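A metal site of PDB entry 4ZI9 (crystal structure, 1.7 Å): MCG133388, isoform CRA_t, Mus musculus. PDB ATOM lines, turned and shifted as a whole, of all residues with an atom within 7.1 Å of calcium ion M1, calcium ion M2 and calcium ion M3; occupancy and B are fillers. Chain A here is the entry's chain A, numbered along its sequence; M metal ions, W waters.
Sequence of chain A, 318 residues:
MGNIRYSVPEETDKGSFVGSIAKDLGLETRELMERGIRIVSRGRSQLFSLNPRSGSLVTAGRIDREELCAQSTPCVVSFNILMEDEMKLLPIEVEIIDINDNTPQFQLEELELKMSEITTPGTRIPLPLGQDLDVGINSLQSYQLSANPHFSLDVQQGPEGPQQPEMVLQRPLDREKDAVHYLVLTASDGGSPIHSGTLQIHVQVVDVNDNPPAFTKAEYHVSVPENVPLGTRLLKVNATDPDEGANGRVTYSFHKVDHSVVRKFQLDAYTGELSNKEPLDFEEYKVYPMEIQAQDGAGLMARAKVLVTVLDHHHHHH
OD1 of Asp 207 is bound to calcium ion M2.
Calcium ion M2 is bound by the side-chain carboxylate (OE2) of Glu 176, at 2.3 Å.
OE1 of Glu 117 is bound to calcium ion M2, 2.3 Å away.
The side-chain carboxylate (OD1) of Asp 210 binds calcium ion M2.
OD1 of Asp 243 is bound to calcium ion M2, at 2.4 Å.
Calcium ion M2 is bound by O of Val 208, at 2.5 Å.
OE1 of Glu 176 is bound to calcium ion M2 (2.6 Å).
Calcium ion M3 is bound by O of Asn 247 (2.3 Å), O of Asn 211 (2.3 Å), OD1 of Asn 209 (2.3 Å), OD2 of Asp 243 (2.4 Å), OD2 of Asp 241 (2.5 Å), OD2 of Asp 296 (2.6 Å) and OD1 of Asp 241 (2.6 Å).
Calcium ion M3 has seven donor atoms within binding distance.
The backbone NH of Glu 117 lies within hydrogen-bond range of the backbone carbonyl oxygen of Val 206 (2.9 Å).
OD1 of Asp 210 sits close to ND2 of Asn 211, 3.2 Å away.
The backbone NH (N) of Arg 175 lies close to the side-chain carboxylate (OE2) of Glu 117 (3.0 Å).
OE1 of Glu 176 sits close to ND2 of Asn 211.
The backbone NH (N) of Glu 244 is in hydrogen-bond range of the side-chain carboxylate (OD2) of Asp 207 (3.0 Å).
The side-chain carboxylate (OD1) of Asp 207 lies close to the guanidinium group (NE) of Arg 175, 3.2 Å away.
The backbone NH (N) of Leu 300 sits at hydrogen-bond distance from the side-chain carboxylate (OD1) of Asp 296 (3.0 Å).
NH2 of Arg 175 sits close to OE2 of Glu 176, at 3.0 Å.
Calcium ion M1 is bound by the side-chain carboxylate (OE1) of Glu 176 (2.3 Å), the side-chain carboxylate (OD1) of Asp 174 (2.3 Å), water W1 (2.4 Å), the side-chain carboxylate (OE2) of Glu 117 (2.4 Å), water W2 (2.5 Å) and the side-chain carboxylate (OD2) of Asp 210 (2.5 Å).
Calcium ion M1 has six donor atoms within binding distance.
The nearest printed residue that does not touch calcium ion M2 is Arg 175 (4.4 Å).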
ATOM      1  N   GLU A 117      -5.217  21.494 -13.025  1.00  0.00           N
ATOM      2  CA  GLU A 117      -6.337  21.271 -13.928  1.00  0.00           C
ATOM      3  C   GLU A 117      -6.685  22.518 -14.734  1.00  0.00           C
ATOM      4  O   GLU A 117      -7.392  22.414 -15.759  1.00  0.00           O
ATOM      5  CB  GLU A 117      -7.556  20.752 -13.167  1.00  0.00           C
ATOM      6  CG  GLU A 117      -8.021  21.619 -12.000  1.00  0.00           C
ATOM      7  CD  GLU A 117      -9.281  21.072 -11.387  1.00  0.00           C
ATOM      8  OE1 GLU A 117      -9.460  21.222 -10.166  1.00  0.00           O
ATOM      9  OE2 GLU A 117     -10.085  20.482 -12.141  1.00  0.00           O
ATOM     10  N   LEU A 173      -7.849  19.818 -18.852  1.00  0.00           N
ATOM     11  CA  LEU A 173      -7.884  18.835 -17.786  1.00  0.00           C
ATOM     12  C   LEU A 173      -9.010  19.109 -16.779  1.00  0.00           C
ATOM     13  O   LEU A 173      -9.548  20.220 -16.719  1.00  0.00           O
ATOM     14  CB  LEU A 173      -6.545  18.820 -17.065  1.00  0.00           C
ATOM     15  CG  LEU A 173      -5.347  18.552 -17.980  1.00  0.00           C
ATOM     16  CD1 LEU A 173      -4.091  18.744 -17.165  1.00  0.00           C
ATOM     17  CD2 LEU A 173      -5.434  17.132 -18.538  1.00  0.00           C
ATOM     18  N   ASP A 174      -9.375  18.088 -15.992  1.00  0.00           N
ATOM     19  CA  ASP A 174     -10.376  18.249 -14.927  1.00  0.00           C
ATOM     20  C   ASP A 174     -10.153  17.188 -13.873  1.00  0.00           C
ATOM     21  O   ASP A 174     -10.487  16.025 -14.080  1.00  0.00           O
ATOM     22  CB  ASP A 174     -11.798  18.162 -15.471  1.00  0.00           C
ATOM     23  CG  ASP A 174     -12.859  18.246 -14.373  1.00  0.00           C
ATOM     24  OD1 ASP A 174     -12.560  18.563 -13.203  1.00  0.00           O
ATOM     25  OD2 ASP A 174     -14.035  17.987 -14.683  1.00  0.00           O
ATOM     26  N   ARG A 175      -9.553  17.570 -12.747  1.00  0.00           N
ATOM     27  CA  ARG A 175      -9.268  16.616 -11.674  1.00  0.00           C
ATOM     28  C   ARG A 175     -10.526  15.913 -11.159  1.00  0.00           C
ATOM     29  O   ARG A 175     -10.448  14.774 -10.729  1.00  0.00           O
ATOM     30  CB  ARG A 175      -8.567  17.331 -10.526  1.00  0.00           C
ATOM     31  CG  ARG A 175      -7.825  16.426  -9.557  1.00  0.00           C
ATOM     32  CD  ARG A 175      -7.788  17.055  -8.186  1.00  0.00           C
ATOM     33  NE  ARG A 175      -9.156  17.206  -7.674  1.00  0.00           N
ATOM     34  CZ  ARG A 175      -9.785  16.296  -6.944  1.00  0.00           C
ATOM     35  NH1 ARG A 175      -9.158  15.176  -6.580  1.00  0.00           N
ATOM     36  NH2 ARG A 175     -11.028  16.497  -6.551  1.00  0.00           N
ATOM     37  N   GLU A 176     -11.680  16.585 -11.197  1.00  0.00           N
ATOM     38  CA  GLU A 176     -12.906  15.953 -10.726  1.00  0.00           C
ATOM     39  C   GLU A 176     -13.423  14.874 -11.703  1.00  0.00           C
ATOM     40  O   GLU A 176     -14.294  14.086 -11.348  1.00  0.00           O
ATOM     41  CB  GLU A 176     -14.002  17.004 -10.479  1.00  0.00           C
ATOM     42  CG  GLU A 176     -13.804  17.798  -9.217  1.00  0.00           C
ATOM     43  CD  GLU A 176     -12.633  18.788  -9.283  1.00  0.00           C
ATOM     44  OE1 GLU A 176     -12.520  19.556 -10.271  1.00  0.00           O
ATOM     45  OE2 GLU A 176     -11.855  18.842  -8.306  1.00  0.00           O
ATOM     46  N   LYS A 177     -12.866  14.826 -12.906  1.00  0.00           N
ATOM     47  CA  LYS A 177     -13.173  13.729 -13.845  1.00  0.00           C
ATOM     48  C   LYS A 177     -12.038  12.710 -13.827  1.00  0.00           C
ATOM     49  O   LYS A 177     -12.252  11.526 -13.617  1.00  0.00           O
ATOM     50  CB  LYS A 177     -13.391  14.272 -15.263  1.00  0.00           C
ATOM     51  CG  LYS A 177     -13.767  13.225 -16.315  1.00  0.00           C
ATOM     52  CD  LYS A 177     -13.826  13.837 -17.726  1.00  0.00           C
ATOM     53  CE  LYS A 177     -14.613  12.968 -18.721  1.00  0.00           C
ATOM     54  NZ  LYS A 177     -13.972  11.655 -19.000  1.00  0.00           N
ATOM     55  N   VAL A 206      -3.357  18.540 -10.660  1.00  0.00           N
ATOM     56  CA  VAL A 206      -3.379  19.288  -9.412  1.00  0.00           C
ATOM     57  C   VAL A 206      -4.702  20.054  -9.273  1.00  0.00           C
ATOM     58  O   VAL A 206      -5.216  20.654 -10.228  1.00  0.00           O
ATOM     59  CB  VAL A 206      -2.182  20.243  -9.316  1.00  0.00           C
ATOM     60  CG1 VAL A 206      -2.195  20.942  -7.995  1.00  0.00           C
ATOM     61  CG2 VAL A 206      -0.904  19.449  -9.440  1.00  0.00           C
ATOM     62  N   ASP A 207      -5.277  19.973  -8.083  1.00  0.00           N
ATOM     63  CA  ASP A 207      -6.605  20.539  -7.854  1.00  0.00           C
ATOM     64  C   ASP A 207      -6.626  22.066  -7.950  1.00  0.00           C
ATOM     65  O   ASP A 207      -5.657  22.729  -7.559  1.00  0.00           O
ATOM     66  CB  ASP A 207      -7.139  20.095  -6.479  1.00  0.00           C
ATOM     67  CG  ASP A 207      -8.615  20.481  -6.254  1.00  0.00           C
ATOM     68  OD1 ASP A 207      -9.450  20.352  -7.175  1.00  0.00           O
ATOM     69  OD2 ASP A 207      -8.929  20.938  -5.153  1.00  0.00           O
ATOM     70  N   VAL A 208      -7.712  22.598  -8.495  1.00  0.00           N
ATOM     71  CA  VAL A 208      -8.061  24.020  -8.348  1.00  0.00           C
ATOM     72  C   VAL A 208      -9.425  24.093  -7.651  1.00  0.00           C
ATOM     73  O   VAL A 208     -10.273  23.218  -7.869  1.00  0.00           O
ATOM     74  CB  VAL A 208      -8.108  24.731  -9.718  1.00  0.00           C
ATOM     75  CG1 VAL A 208      -8.671  26.152  -9.590  1.00  0.00           C
ATOM     76  CG2 VAL A 208      -6.704  24.749 -10.366  1.00  0.00           C
ATOM     77  N   ASN A 209      -9.658  25.113  -6.815  1.00  0.00           N
ATOM     78  CA  ASN A 209     -10.987  25.245  -6.224  1.00  0.00           C
ATOM     79  C   ASN A 209     -11.922  25.762  -7.297  1.00  0.00           C
ATOM     80  O   ASN A 209     -12.136  26.967  -7.389  1.00  0.00           O
ATOM     81  CB  ASN A 209     -10.999  26.182  -5.026  1.00  0.00           C
ATOM     82  CG  ASN A 209     -12.310  26.072  -4.242  1.00  0.00           C
ATOM     83  OD1 ASN A 209     -12.954  24.993  -4.225  1.00  0.00           O
ATOM     84  ND2 ASN A 209     -12.730  27.172  -3.612  1.00  0.00           N
ATOM     85  N   ASP A 210     -12.472  24.876  -8.095  1.00  0.00           N
ATOM     86  CA  ASP A 210     -13.315  25.330  -9.196  1.00  0.00           C
ATOM     87  C   ASP A 210     -14.753  24.809  -9.106  1.00  0.00           C
ATOM     88  O   ASP A 210     -15.511  24.867 -10.087  1.00  0.00           O
ATOM     89  CB  ASP A 210     -12.677  24.990 -10.558  1.00  0.00           C
ATOM     90  CG  ASP A 210     -12.380  23.499 -10.754  1.00  0.00           C
ATOM     91  OD1 ASP A 210     -12.252  22.719  -9.776  1.00  0.00           O
ATOM     92  OD2 ASP A 210     -12.252  23.101 -11.931  1.00  0.00           O
ATOM     93  N   ASN A 211     -15.131  24.302  -7.941  1.00  0.00           N
ATOM     94  CA  ASN A 211     -16.523  23.922  -7.689  1.00  0.00           C
ATOM     95  C   ASN A 211     -16.983  24.548  -6.390  1.00  0.00           C
ATOM     96  O   ASN A 211     -16.302  24.427  -5.375  1.00  0.00           O
ATOM     97  CB  ASN A 211     -16.720  22.415  -7.582  1.00  0.00           C
ATOM     98  CG  ASN A 211     -16.382  21.683  -8.857  1.00  0.00           C
ATOM     99  OD1 ASN A 211     -17.252  21.417  -9.680  1.00  0.00           O
ATOM    100  ND2 ASN A 211     -15.100  21.366  -9.035  1.00  0.00           N
ATOM    101  N   PRO A 212     -18.133  25.217  -6.420  1.00  0.00           N
ATOM    102  CA  PRO A 212     -18.752  25.654  -5.169  1.00  0.00           C
ATOM    103  C   PRO A 212     -19.400  24.475  -4.451  1.00  0.00           C
ATOM    104  O   PRO A 212     -19.719  23.472  -5.061  1.00  0.00           O
ATOM    105  CB  PRO A 212     -19.809  26.649  -5.634  1.00  0.00           C
ATOM    106  CG  PRO A 212     -20.287  26.020  -6.919  1.00  0.00           C
ATOM    107  CD  PRO A 212     -19.012  25.473  -7.577  1.00  0.00           C
ATOM    108  N   PRO A 213     -19.618  24.605  -3.135  1.00  0.00           N
ATOM    109  CA  PRO A 213     -20.445  23.567  -2.498  1.00  0.00           C
ATOM    110  C   PRO A 213     -21.869  23.553  -3.091  1.00  0.00           C
ATOM    111  O   PRO A 213     -22.258  24.456  -3.826  1.00  0.00           O
ATOM    112  CB  PRO A 213     -20.468  23.977  -1.027  1.00  0.00           C
ATOM    113  CG  PRO A 213     -19.401  25.029  -0.874  1.00  0.00           C
ATOM    114  CD  PRO A 213     -19.216  25.665  -2.208  1.00  0.00           C
ATOM    115  N   THR A 240     -22.349  19.295  -0.333  1.00  0.00           N
ATOM    116  CA  THR A 240     -21.214  18.502  -0.798  1.00  0.00           C
ATOM    117  C   THR A 240     -20.353  19.371  -1.703  1.00  0.00           C
ATOM    118  O   THR A 240     -20.815  20.390  -2.221  1.00  0.00           O
ATOM    119  CB  THR A 240     -21.678  17.260  -1.545  1.00  0.00           C
ATOM    120  OG1 THR A 240     -22.544  17.634  -2.621  1.00  0.00           O
ATOM    121  CG2 THR A 240     -22.434  16.326  -0.607  1.00  0.00           C
ATOM    122  N   ASP A 241     -19.093  18.968  -1.890  1.00  0.00           N
ATOM    123  CA  ASP A 241     -18.137  19.755  -2.668  1.00  0.00           C
ATOM    124  C   ASP A 241     -17.067  18.797  -3.211  1.00  0.00           C
ATOM    125  O   ASP A 241     -16.390  18.133  -2.436  1.00  0.00           O
ATOM    126  CB  ASP A 241     -17.503  20.838  -1.829  1.00  0.00           C
ATOM    127  CG  ASP A 241     -16.677  21.823  -2.652  1.00  0.00           C
ATOM    128  OD1 ASP A 241     -15.924  21.405  -3.576  1.00  0.00           O
ATOM    129  OD2 ASP A 241     -16.798  23.034  -2.375  1.00  0.00           O
ATOM    130  N   PRO A 242     -16.940  18.711  -4.538  1.00  0.00           N
ATOM    131  CA  PRO A 242     -16.116  17.666  -5.163  1.00  0.00           C
ATOM    132  C   PRO A 242     -14.620  18.010  -5.270  1.00  0.00           C
ATOM    133  O   PRO A 242     -13.848  17.182  -5.732  1.00  0.00           O
ATOM    134  CB  PRO A 242     -16.741  17.535  -6.546  1.00  0.00           C
ATOM    135  CG  PRO A 242     -17.267  18.907  -6.828  1.00  0.00           C
ATOM    136  CD  PRO A 242     -17.704  19.489  -5.529  1.00  0.00           C
ATOM    137  N   ASP A 243     -14.224  19.203  -4.868  1.00  0.00           N
ATOM    138  CA  ASP A 243     -12.810  19.559  -4.895  1.00  0.00           C
ATOM    139  C   ASP A 243     -12.053  18.829  -3.786  1.00  0.00           C
ATOM    140  O   ASP A 243     -12.666  18.182  -2.916  1.00  0.00           O
ATOM    141  CB  ASP A 243     -12.623  21.083  -4.764  1.00  0.00           C
ATOM    142  CG  ASP A 243     -13.206  21.834  -5.933  1.00  0.00           C
ATOM    143  OD1 ASP A 243     -12.970  21.442  -7.094  1.00  0.00           O
ATOM    144  OD2 ASP A 243     -13.946  22.785  -5.685  1.00  0.00           O
ATOM    145  N   GLU A 244     -10.726  18.948  -3.807  1.00  0.00           N
ATOM    146  CA  GLU A 244      -9.841  18.157  -2.949  1.00  0.00           C
ATOM    147  C   GLU A 244      -9.423  18.906  -1.684  1.00  0.00           C
ATOM    148  O   GLU A 244      -9.143  20.103  -1.717  1.00  0.00           O
ATOM    149  CB  GLU A 244      -8.590  17.739  -3.734  1.00  0.00           C
ATOM    150  CG  GLU A 244      -7.573  16.925  -2.939  1.00  0.00           C
ATOM    151  CD  GLU A 244      -6.361  16.491  -3.777  1.00  0.00           C
ATOM    152  OE1 GLU A 244      -6.048  17.178  -4.772  1.00  0.00           O
ATOM    153  OE2 GLU A 244      -5.743  15.463  -3.454  1.00  0.00           O
ATOM    154  N   ALA A 246      -8.988  21.035   1.509  1.00  0.00           N
ATOM    155  CA  ALA A 246      -9.633  22.251   1.983  1.00  0.00           C
ATOM    156  C   ALA A 246     -10.598  22.836   0.953  1.00  0.00           C
ATOM    157  O   ALA A 246     -11.598  23.459   1.330  1.00  0.00           O
ATOM    158  CB  ALA A 246      -8.598  23.271   2.362  1.00  0.00           C
ATOM    159  N   ASN A 247     -10.288  22.652  -0.318  1.00  0.00           N
ATOM    160  CA  ASN A 247     -11.165  23.136  -1.395  1.00  0.00           C
ATOM    161  C   ASN A 247     -12.552  22.483  -1.411  1.00  0.00           C
ATOM    162  O   ASN A 247     -13.503  23.063  -1.955  1.00  0.00           O
ATOM    163  CB  ASN A 247     -10.490  22.935  -2.753  1.00  0.00           C
ATOM    164  CG  ASN A 247      -9.192  23.677  -2.865  1.00  0.00           C
ATOM    165  OD1 ASN A 247      -8.993  24.692  -2.202  1.00  0.00           O
ATOM    166  ND2 ASN A 247      -8.298  23.195  -3.727  1.00  0.00           N
ATOM    167  N   GLY A 248     -12.651  21.286  -0.838  1.00  0.00           N
ATOM    168  CA  GLY A 248     -13.900  20.536  -0.775  1.00  0.00           C
ATOM    169  C   GLY A 248     -14.483  20.417   0.638  1.00  0.00           C
ATOM    170  O   GLY A 248     -15.477  19.720   0.861  1.00  0.00           O
ATOM    171  N   ARG A 249     -13.839  21.073   1.594  1.00  0.00           N
ATOM    172  CA  ARG A 249     -14.284  21.022   2.989  1.00  0.00           C
ATOM    173  C   ARG A 249     -15.223  22.188   3.289  1.00  0.00           C
ATOM    174  O   ARG A 249     -14.845  23.357   3.153  1.00  0.00           O
ATOM    175  CB  ARG A 249     -13.060  21.064   3.921  1.00  0.00           C
ATOM    176  CG  ARG A 249     -13.344  20.899   5.401  1.00  0.00           C
ATOM    177  CD  ARG A 249     -12.032  20.585   6.117  1.00  0.00           C
ATOM    178  NE  ARG A 249     -11.273  19.541   5.422  1.00  0.00           N
ATOM    179  CZ  ARG A 249     -10.026  19.673   4.963  1.00  0.00           C
ATOM    180  NH1 ARG A 249      -9.368  20.816   5.115  1.00  0.00           N
ATOM    181  NH2 ARG A 249      -9.437  18.647   4.347  1.00  0.00           N
ATOM    182  N   VAL A 250     -16.452  21.881   3.695  1.00  0.00           N
ATOM    183  CA  VAL A 250     -17.440  22.946   3.822  1.00  0.00           C
ATOM    184  C   VAL A 250     -17.898  23.192   5.253  1.00  0.00           C
ATOM    185  O   VAL A 250     -18.044  22.272   6.070  1.00  0.00           O
ATOM    186  CB  VAL A 250     -18.671  22.670   2.915  1.00  0.00           C
ATOM    187  CG1 VAL A 250     -18.399  21.526   1.970  1.00  0.00           C
ATOM    188  CG2 VAL A 250     -19.920  22.435   3.706  1.00  0.00           C
ATOM    189  N   ASP A 296     -16.767  26.583   1.187  1.00  0.00           N
ATOM    190  CA  ASP A 296     -15.628  25.657   1.158  1.00  0.00           C
ATOM    191  C   ASP A 296     -14.424  26.386   1.768  1.00  0.00           C
ATOM    192  O   ASP A 296     -14.551  27.482   2.282  1.00  0.00           O
ATOM    193  CB  ASP A 296     -15.317  25.132  -0.259  1.00  0.00           C
ATOM    194  CG  ASP A 296     -14.913  26.221  -1.244  1.00  0.00           C
ATOM    195  OD1 ASP A 296     -14.375  27.300  -0.863  1.00  0.00           O
ATOM    196  OD2 ASP A 296     -15.124  25.969  -2.454  1.00  0.00           O
ATOM    197  N   GLY A 297     -13.252  25.773   1.697  1.00  0.00           N
ATOM    198  CA  GLY A 297     -12.128  26.359   2.392  1.00  0.00           C
ATOM    199  C   GLY A 297     -11.387  27.416   1.596  1.00  0.00           C
ATOM    200  O   GLY A 297     -10.347  27.891   2.041  1.00  0.00           O
ATOM    201  N   ALA A 298     -11.918  27.807   0.435  1.00  0.00           N
ATOM    202  CA  ALA A 298     -11.159  28.710  -0.443  1.00  0.00           C
ATOM    203  C   ALA A 298     -12.041  29.687  -1.231  1.00  0.00           C
ATOM    204  O   ALA A 298     -11.764  29.953  -2.407  1.00  0.00           O
ATOM    205  CB  ALA A 298     -10.264  27.892  -1.414  1.00  0.00           C
ATOM    206  N   LEU A 300     -15.440  29.764  -2.192  1.00  0.00           N
ATOM    207  CA  LEU A 300     -16.645  29.512  -2.968  1.00  0.00           C
ATOM    208  C   LEU A 300     -17.764  29.150  -1.989  1.00  0.00           C
ATOM    209  O   LEU A 300     -17.522  28.671  -0.888  1.00  0.00           O
ATOM    210  CB  LEU A 300     -16.437  28.416  -4.018  1.00  0.00           C
ATOM    211  CG  LEU A 300     -15.469  28.758  -5.156  1.00  0.00           C
ATOM    212  CD1 LEU A 300     -15.384  27.595  -6.104  1.00  0.00           C
ATOM    213  CD2 LEU A 300     -15.935  30.018  -5.888  1.00  0.00           C
HETATM  214 CA    CA M   1     -12.461  20.657 -12.262  1.00  0.00          CA
HETATM  215 CA    CA M   2     -11.144  21.036  -8.569  1.00  0.00          CA
HETATM  216 CA    CA M   3     -14.854  23.747  -3.695  1.00  0.00          CA
HETATM  217  O   HOH W   1     -12.475  21.436 -14.482  1.00  0.00           O
HETATM  218  O   HOH W   2     -14.868  21.127 -12.097  1.00  0.00           O
